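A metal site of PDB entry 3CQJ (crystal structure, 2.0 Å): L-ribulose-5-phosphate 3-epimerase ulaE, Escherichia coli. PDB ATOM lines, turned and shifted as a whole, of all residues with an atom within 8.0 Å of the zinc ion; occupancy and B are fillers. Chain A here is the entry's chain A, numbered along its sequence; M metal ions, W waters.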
ATOM      1  N   TYR A  22     -19.994  12.121  12.289  1.00  0.00           N
ATOM      2  CA  TYR A  22     -18.574  11.982  12.626  1.00  0.00           C
ATOM      3  C   TYR A  22     -18.217  10.509  12.892  1.00  0.00           C
ATOM      4  O   TYR A  22     -18.939   9.804  13.613  1.00  0.00           O
ATOM      5  CB  TYR A  22     -18.250  12.845  13.848  1.00  0.00           C
ATOM      6  CG  TYR A  22     -16.776  13.119  14.095  1.00  0.00           C
ATOM      7  CD1 TYR A  22     -15.937  13.505  13.050  1.00  0.00           C
ATOM      8  CD2 TYR A  22     -16.234  13.023  15.378  1.00  0.00           C
ATOM      9  CE1 TYR A  22     -14.591  13.762  13.254  1.00  0.00           C
ATOM     10  CE2 TYR A  22     -14.873  13.283  15.608  1.00  0.00           C
ATOM     11  CZ  TYR A  22     -14.068  13.652  14.542  1.00  0.00           C
ATOM     12  OH  TYR A  22     -12.732  13.909  14.748  1.00  0.00           O
ATOM     13  N   GLU A  48     -17.816  11.396   8.038  1.00  0.00           N
ATOM     14  CA  GLU A  48     -16.521  12.053   8.006  1.00  0.00           C
ATOM     15  C   GLU A  48     -15.488  11.187   8.708  1.00  0.00           C
ATOM     16  O   GLU A  48     -15.648  10.850   9.873  1.00  0.00           O
ATOM     17  CB  GLU A  48     -16.604  13.436   8.634  1.00  0.00           C
ATOM     18  CG  GLU A  48     -15.266  14.115   8.859  1.00  0.00           C
ATOM     19  CD  GLU A  48     -15.458  15.611   9.039  1.00  0.00           C
ATOM     20  OE1 GLU A  48     -15.369  16.080  10.191  1.00  0.00           O
ATOM     21  OE2 GLU A  48     -15.746  16.294   8.032  1.00  0.00           O
ATOM     22  N   CYS A  86     -11.309  14.595   8.818  1.00  0.00           N
ATOM     23  CA  CYS A  86     -10.854  15.510   9.863  1.00  0.00           C
ATOM     24  C   CYS A  86      -9.419  15.129  10.193  1.00  0.00           C
ATOM     25  O   CYS A  86      -9.160  14.021  10.660  1.00  0.00           O
ATOM     26  CB  CYS A  86     -11.727  15.363  11.110  1.00  0.00           C
ATOM     27  SG  CYS A  86     -10.979  16.108  12.600  1.00  0.00           S
ATOM     28  N   GLN A 126     -10.196  18.549   6.283  1.00  0.00           N
ATOM     29  CA  GLN A 126     -10.355  19.578   7.315  1.00  0.00           C
ATOM     30  C   GLN A 126      -9.091  19.682   8.155  1.00  0.00           C
ATOM     31  O   GLN A 126      -8.689  18.715   8.828  1.00  0.00           O
ATOM     32  CB  GLN A 126     -11.555  19.261   8.210  1.00  0.00           C
ATOM     33  CG  GLN A 126     -11.909  20.375   9.179  1.00  0.00           C
ATOM     34  CD  GLN A 126     -12.958  19.968  10.181  1.00  0.00           C
ATOM     35  OE1 GLN A 126     -12.899  18.851  10.718  1.00  0.00           O
ATOM     36  NE2 GLN A 126     -13.920  20.857  10.453  1.00  0.00           N
ATOM     37  N   GLU A 166     -10.689  24.509   9.792  1.00  0.00           N
ATOM     38  CA  GLU A 166     -11.738  24.515  10.793  1.00  0.00           C
ATOM     39  C   GLU A 166     -11.608  25.729  11.700  1.00  0.00           C
ATOM     40  O   GLU A 166     -10.500  26.158  12.026  1.00  0.00           O
ATOM     41  CB  GLU A 166     -11.722  23.244  11.656  1.00  0.00           C
ATOM     42  CG  GLU A 166     -12.917  23.219  12.634  1.00  0.00           C
ATOM     43  CD  GLU A 166     -12.957  22.014  13.535  1.00  0.00           C
ATOM     44  OE1 GLU A 166     -11.888  21.443  13.831  1.00  0.00           O
ATOM     45  OE2 GLU A 166     -14.082  21.646  13.969  1.00  0.00           O
ATOM     46  N   ILE A 167     -12.748  26.270  12.125  1.00  0.00           N
ATOM     47  CA  ILE A 167     -12.779  27.272  13.189  1.00  0.00           C
ATOM     48  C   ILE A 167     -12.598  26.525  14.516  1.00  0.00           C
ATOM     49  O   ILE A 167     -13.335  25.583  14.811  1.00  0.00           O
ATOM     50  CB  ILE A 167     -14.072  28.126  13.115  1.00  0.00           C
ATOM     51  CG1 ILE A 167     -13.944  29.241  12.058  1.00  0.00           C
ATOM     52  CG2 ILE A 167     -14.391  28.781  14.459  1.00  0.00           C
ATOM     53  CD1 ILE A 167     -13.584  28.807  10.626  1.00  0.00           C
ATOM     54  N   MET A 168     -11.632  26.968  15.325  1.00  0.00           N
ATOM     55  CA  MET A 168     -11.001  26.125  16.357  1.00  0.00           C
ATOM     56  C   MET A 168     -11.284  26.473  17.807  1.00  0.00           C
ATOM     57  O   MET A 168     -11.744  27.590  18.145  1.00  0.00           O
ATOM     58  CB  MET A 168      -9.467  26.147  16.189  1.00  0.00           C
ATOM     59  CG  MET A 168      -8.938  25.679  14.855  1.00  0.00           C
ATOM     60  SD  MET A 168      -9.374  23.978  14.469  1.00  0.00           S
ATOM     61  CE  MET A 168      -8.642  23.103  15.848  1.00  0.00           C
ATOM     62  N   ASP A 169     -10.943  25.507  18.663  1.00  0.00           N
ATOM     63  CA  ASP A 169     -10.937  25.646  20.110  1.00  0.00           C
ATOM     64  C   ASP A 169      -9.628  26.298  20.580  1.00  0.00           C
ATOM     65  O   ASP A 169      -9.113  25.989  21.668  1.00  0.00           O
ATOM     66  CB  ASP A 169     -11.105  24.254  20.764  1.00  0.00           C
ATOM     67  CG  ASP A 169      -9.958  23.289  20.434  1.00  0.00           C
ATOM     68  OD1 ASP A 169      -9.330  23.400  19.360  1.00  0.00           O
ATOM     69  OD2 ASP A 169      -9.705  22.372  21.255  1.00  0.00           O
ATOM     70  N   TYR A 194     -14.149  25.694   6.883  1.00  0.00           N
ATOM     71  CA  TYR A 194     -14.972  24.633   7.436  1.00  0.00           C
ATOM     72  C   TYR A 194     -15.376  25.064   8.847  1.00  0.00           C
ATOM     73  O   TYR A 194     -14.803  24.590   9.827  1.00  0.00           O
ATOM     74  CB  TYR A 194     -14.158  23.336   7.485  1.00  0.00           C
ATOM     75  CG  TYR A 194     -14.982  22.070   7.635  1.00  0.00           C
ATOM     76  CD1 TYR A 194     -14.539  20.872   7.065  1.00  0.00           C
ATOM     77  CD2 TYR A 194     -16.190  22.062   8.354  1.00  0.00           C
ATOM     78  CE1 TYR A 194     -15.262  19.690   7.225  1.00  0.00           C
ATOM     79  CE2 TYR A 194     -16.926  20.885   8.495  1.00  0.00           C
ATOM     80  CZ  TYR A 194     -16.463  19.709   7.926  1.00  0.00           C
ATOM     81  OH  TYR A 194     -17.178  18.526   8.070  1.00  0.00           O
ATOM     82  N   PRO A 195     -16.373  25.950   8.966  1.00  0.00           N
ATOM     83  CA  PRO A 195     -16.708  26.427  10.310  1.00  0.00           C
ATOM     84  C   PRO A 195     -17.323  25.337  11.192  1.00  0.00           C
ATOM     85  O   PRO A 195     -18.030  24.453  10.705  1.00  0.00           O
ATOM     86  CB  PRO A 195     -17.743  27.537  10.058  1.00  0.00           C
ATOM     87  CG  PRO A 195     -17.762  27.773   8.594  1.00  0.00           C
ATOM     88  CD  PRO A 195     -17.205  26.576   7.911  1.00  0.00           C
ATOM     89  N   ASP A 196     -16.989  25.409  12.470  1.00  0.00           N
ATOM     90  CA  ASP A 196     -17.639  24.601  13.486  1.00  0.00           C
ATOM     91  C   ASP A 196     -18.442  25.594  14.296  1.00  0.00           C
ATOM     92  O   ASP A 196     -17.859  26.453  14.943  1.00  0.00           O
ATOM     93  CB  ASP A 196     -16.604  23.871  14.338  1.00  0.00           C
ATOM     94  CG  ASP A 196     -17.233  23.085  15.485  1.00  0.00           C
ATOM     95  OD1 ASP A 196     -18.032  23.669  16.260  1.00  0.00           O
ATOM     96  OD2 ASP A 196     -16.916  21.881  15.614  1.00  0.00           O
ATOM     97  N   ILE A 197     -19.767  25.518  14.249  1.00  0.00           N
ATOM     98  CA  ILE A 197     -20.592  26.534  14.873  1.00  0.00           C
ATOM     99  C   ILE A 197     -20.507  26.485  16.400  1.00  0.00           C
ATOM    100  O   ILE A 197     -20.757  27.487  17.060  1.00  0.00           O
ATOM    101  CB  ILE A 197     -22.077  26.538  14.361  1.00  0.00           C
ATOM    102  CG1 ILE A 197     -22.831  25.257  14.746  1.00  0.00           C
ATOM    103  CG2 ILE A 197     -22.135  26.817  12.848  1.00  0.00           C
ATOM    104  CD1 ILE A 197     -24.294  25.228  14.240  1.00  0.00           C
ATOM    105  N   GLY A 198     -20.133  25.332  16.938  1.00  0.00           N
ATOM    106  CA  GLY A 198     -19.812  25.211  18.347  1.00  0.00           C
ATOM    107  C   GLY A 198     -18.594  26.035  18.727  1.00  0.00           C
ATOM    108  O   GLY A 198     -18.673  26.902  19.598  1.00  0.00           O
ATOM    109  N   ASN A 199     -17.469  25.769  18.074  1.00  0.00           N
ATOM    110  CA  ASN A 199     -16.240  26.530  18.322  1.00  0.00           C
ATOM    111  C   ASN A 199     -16.412  28.028  18.081  1.00  0.00           C
ATOM    112  O   ASN A 199     -15.864  28.844  18.817  1.00  0.00           O
ATOM    113  CB  ASN A 199     -15.103  25.994  17.458  1.00  0.00           C
ATOM    114  CG  ASN A 199     -14.722  24.567  17.809  1.00  0.00           C
ATOM    115  OD1 ASN A 199     -15.124  24.042  18.840  1.00  0.00           O
ATOM    116  ND2 ASN A 199     -13.895  23.948  16.961  1.00  0.00           N
ATOM    117  N   VAL A 221     -19.951  22.372   7.268  1.00  0.00           N
ATOM    118  CA  VAL A 221     -20.241  22.941   8.588  1.00  0.00           C
ATOM    119  C   VAL A 221     -20.302  21.812   9.621  1.00  0.00           C
ATOM    120  O   VAL A 221     -21.066  20.837   9.448  1.00  0.00           O
ATOM    121  CB  VAL A 221     -21.579  23.753   8.605  1.00  0.00           C
ATOM    122  CG1 VAL A 221     -21.839  24.343   9.989  1.00  0.00           C
ATOM    123  CG2 VAL A 221     -21.567  24.867   7.517  1.00  0.00           C
ATOM    124  N   HIS A 222     -19.463  21.924  10.652  1.00  0.00           N
ATOM    125  CA  HIS A 222     -19.544  21.067  11.847  1.00  0.00           C
ATOM    126  C   HIS A 222     -20.629  21.583  12.777  1.00  0.00           C
ATOM    127  O   HIS A 222     -20.687  22.766  13.105  1.00  0.00           O
ATOM    128  CB  HIS A 222     -18.200  21.052  12.600  1.00  0.00           C
ATOM    129  CG  HIS A 222     -17.276  19.955  12.191  1.00  0.00           C
ATOM    130  ND1 HIS A 222     -16.135  19.627  12.896  1.00  0.00           N
ATOM    131  CD2 HIS A 222     -17.318  19.093  11.138  1.00  0.00           C
ATOM    132  CE1 HIS A 222     -15.518  18.620  12.305  1.00  0.00           C
ATOM    133  NE2 HIS A 222     -16.215  18.276  11.239  1.00  0.00           N
ATOM    134  N   VAL A 223     -21.496  20.664  13.206  1.00  0.00           N
ATOM    135  CA  VAL A 223     -22.627  20.965  14.073  1.00  0.00           C
ATOM    136  C   VAL A 223     -22.401  20.323  15.439  1.00  0.00           C
ATOM    137  O   VAL A 223     -22.458  19.090  15.574  1.00  0.00           O
ATOM    138  CB  VAL A 223     -23.966  20.467  13.447  1.00  0.00           C
ATOM    139  CG1 VAL A 223     -25.131  20.655  14.397  1.00  0.00           C
ATOM    140  CG2 VAL A 223     -24.241  21.165  12.098  1.00  0.00           C
ATOM    141  N   LYS A 224     -22.144  21.154  16.438  1.00  0.00           N
ATOM    142  CA  LYS A 224     -22.012  20.702  17.820  1.00  0.00           C
ATOM    143  C   LYS A 224     -22.244  21.836  18.795  1.00  0.00           C
ATOM    144  O   LYS A 224     -22.135  23.012  18.420  1.00  0.00           O
ATOM    145  CB  LYS A 224     -20.673  20.017  18.077  1.00  0.00           C
ATOM    146  CG  LYS A 224     -19.464  20.908  17.991  1.00  0.00           C
ATOM    147  CD  LYS A 224     -18.270  20.272  18.721  1.00  0.00           C
ATOM    148  CE  LYS A 224     -17.396  21.353  19.325  1.00  0.00           C
ATOM    149  NZ  LYS A 224     -16.025  21.475  18.747  1.00  0.00           N
ATOM    150  N   PHE A 231     -15.173  22.607  24.733  1.00  0.00           N
ATOM    151  CA  PHE A 231     -15.330  22.419  23.287  1.00  0.00           C
ATOM    152  C   PHE A 231     -15.651  20.978  22.897  1.00  0.00           C
ATOM    153  O   PHE A 231     -15.831  20.673  21.713  1.00  0.00           O
ATOM    154  CB  PHE A 231     -14.064  22.877  22.560  1.00  0.00           C
ATOM    155  CG  PHE A 231     -13.705  24.319  22.814  1.00  0.00           C
ATOM    156  CD1 PHE A 231     -14.202  25.333  22.001  1.00  0.00           C
ATOM    157  CD2 PHE A 231     -12.848  24.661  23.861  1.00  0.00           C
ATOM    158  CE1 PHE A 231     -13.865  26.658  22.227  1.00  0.00           C
ATOM    159  CE2 PHE A 231     -12.511  25.987  24.087  1.00  0.00           C
ATOM    160  CZ  PHE A 231     -13.019  26.992  23.270  1.00  0.00           C
ATOM    161  N   LEU A 260     -22.335  18.312   9.224  1.00  0.00           N
ATOM    162  CA  LEU A 260     -21.788  17.136   9.881  1.00  0.00           C
ATOM    163  C   LEU A 260     -22.008  17.263  11.374  1.00  0.00           C
ATOM    164  O   LEU A 260     -21.561  18.243  12.016  1.00  0.00           O
ATOM    165  CB  LEU A 260     -20.286  17.020   9.567  1.00  0.00           C
ATOM    166  CG  LEU A 260     -19.373  15.878  10.051  1.00  0.00           C
ATOM    167  CD1 LEU A 260     -19.006  15.979  11.530  1.00  0.00           C
ATOM    168  CD2 LEU A 260     -19.971  14.538   9.718  1.00  0.00           C
ATOM    169  N   ILE A 261     -22.721  16.292  11.928  1.00  0.00           N
ATOM    170  CA  ILE A 261     -22.956  16.212  13.359  1.00  0.00           C
ATOM    171  C   ILE A 261     -21.731  15.630  14.034  1.00  0.00           C
ATOM    172  O   ILE A 261     -21.361  14.464  13.818  1.00  0.00           O
ATOM    173  CB  ILE A 261     -24.212  15.369  13.714  1.00  0.00           C
ATOM    174  CG1 ILE A 261     -25.473  16.009  13.132  1.00  0.00           C
ATOM    175  CG2 ILE A 261     -24.316  15.192  15.250  1.00  0.00           C
ATOM    176  CD1 ILE A 261     -26.760  15.160  13.306  1.00  0.00           C
ATOM    177  N   GLU A 262     -21.108  16.458  14.858  1.00  0.00           N
ATOM    178  CA  GLU A 262     -19.889  16.081  15.534  1.00  0.00           C
ATOM    179  C   GLU A 262     -20.173  15.718  16.990  1.00  0.00           C
ATOM    180  O   GLU A 262     -20.567  16.565  17.799  1.00  0.00           O
ATOM    181  CB  GLU A 262     -18.869  17.212  15.446  1.00  0.00           C
ATOM    182  CG  GLU A 262     -17.670  16.969  16.327  1.00  0.00           C
ATOM    183  CD  GLU A 262     -16.517  17.893  16.030  1.00  0.00           C
ATOM    184  OE1 GLU A 262     -16.754  18.984  15.453  1.00  0.00           O
ATOM    185  OE2 GLU A 262     -15.376  17.528  16.364  1.00  0.00           O
ATOM    186  N   MET A 263     -19.966  14.443  17.302  1.00  0.00           N
ATOM    187  CA  MET A 263     -20.119  13.933  18.665  1.00  0.00           C
ATOM    188  C   MET A 263     -19.211  12.720  18.870  1.00  0.00           C
ATOM    189  O   MET A 263     -18.690  12.160  17.894  1.00  0.00           O
ATOM    190  CB  MET A 263     -21.592  13.608  18.965  1.00  0.00           C
ATOM    191  CG  MET A 263     -22.265  12.694  17.949  1.00  0.00           C
ATOM    192  SD  MET A 263     -24.058  12.533  18.183  1.00  0.00           S
ATOM    193  CE  MET A 263     -24.156  11.850  19.851  1.00  0.00           C
ATOM    194  N   TRP A 264     -19.001  12.337  20.124  1.00  0.00           N
ATOM    195  CA  TRP A 264     -18.061  11.260  20.475  1.00  0.00           C
ATOM    196  C   TRP A 264     -18.735  10.092  21.173  1.00  0.00           C
ATOM    197  O   TRP A 264     -18.159   9.499  22.094  1.00  0.00           O
ATOM    198  CB  TRP A 264     -16.917  11.810  21.337  1.00  0.00           C
ATOM    199  CG  TRP A 264     -15.968  12.694  20.602  1.00  0.00           C
ATOM    200  CD1 TRP A 264     -14.775  12.334  20.041  1.00  0.00           C
ATOM    201  CD2 TRP A 264     -16.142  14.089  20.329  1.00  0.00           C
ATOM    202  NE1 TRP A 264     -14.186  13.429  19.429  1.00  0.00           N
ATOM    203  CE2 TRP A 264     -15.007  14.520  19.605  1.00  0.00           C
ATOM    204  CE3 TRP A 264     -17.139  15.024  20.644  1.00  0.00           C
ATOM    205  CZ2 TRP A 264     -14.840  15.836  19.176  1.00  0.00           C
ATOM    206  CZ3 TRP A 264     -16.981  16.347  20.223  1.00  0.00           C
ATOM    207  CH2 TRP A 264     -15.845  16.728  19.497  1.00  0.00           C
HETATM  208 ZN    ZN M   1     -15.623  20.543  14.767  1.00  0.00          ZN
HETATM  209  O   HOH W   1     -13.933  19.670  16.176  1.00  0.00           O
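Within 4 Å of the zinc ion: Glu 166, Asp 196, His 222 and Glu 262.
OD2 of Asp 196 is bound to the zinc ion (2.0 Å). The zinc ion is bound by the side-chain carboxylate (OE1) of Glu 262, 2.0 Å away. OE2 of Glu 166 is bound to the zinc ion. ND1 of His 222 is bound to the zinc ion, at 2.1 Å. Water W1 binds the zinc ion (2.4 Å).
The side-chain amino group (NZ) of Lys 224 is in salt-bridge range of the side-chain carboxylate (OD1) of Asp 196 (3.9 Å). The backbone NH of Asn 199 sits at hydrogen-bond distance from the side-chain carboxylate of Asp 196, at 2.8 Å. O of Val 223 lies within hydrogen-bond range of N of Glu 262 (3.0 Å). NE2 of His 222 sits close to OE1 of Gln 126. O of Pro 195 sits at hydrogen-bond distance from N of His 222 (2.9 Å). OE1 of Glu 48 is in hydrogen-bond range of NE2 of His 222 (2.6 Å). The side-chain hydroxyl (OH) of Tyr 194 sits close to a ring nitrogen (NE2) of His 222, at 3.3 Å. N of Ile 197 lies within hydrogen-bond range of O of His 222, at 3.1 Å.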
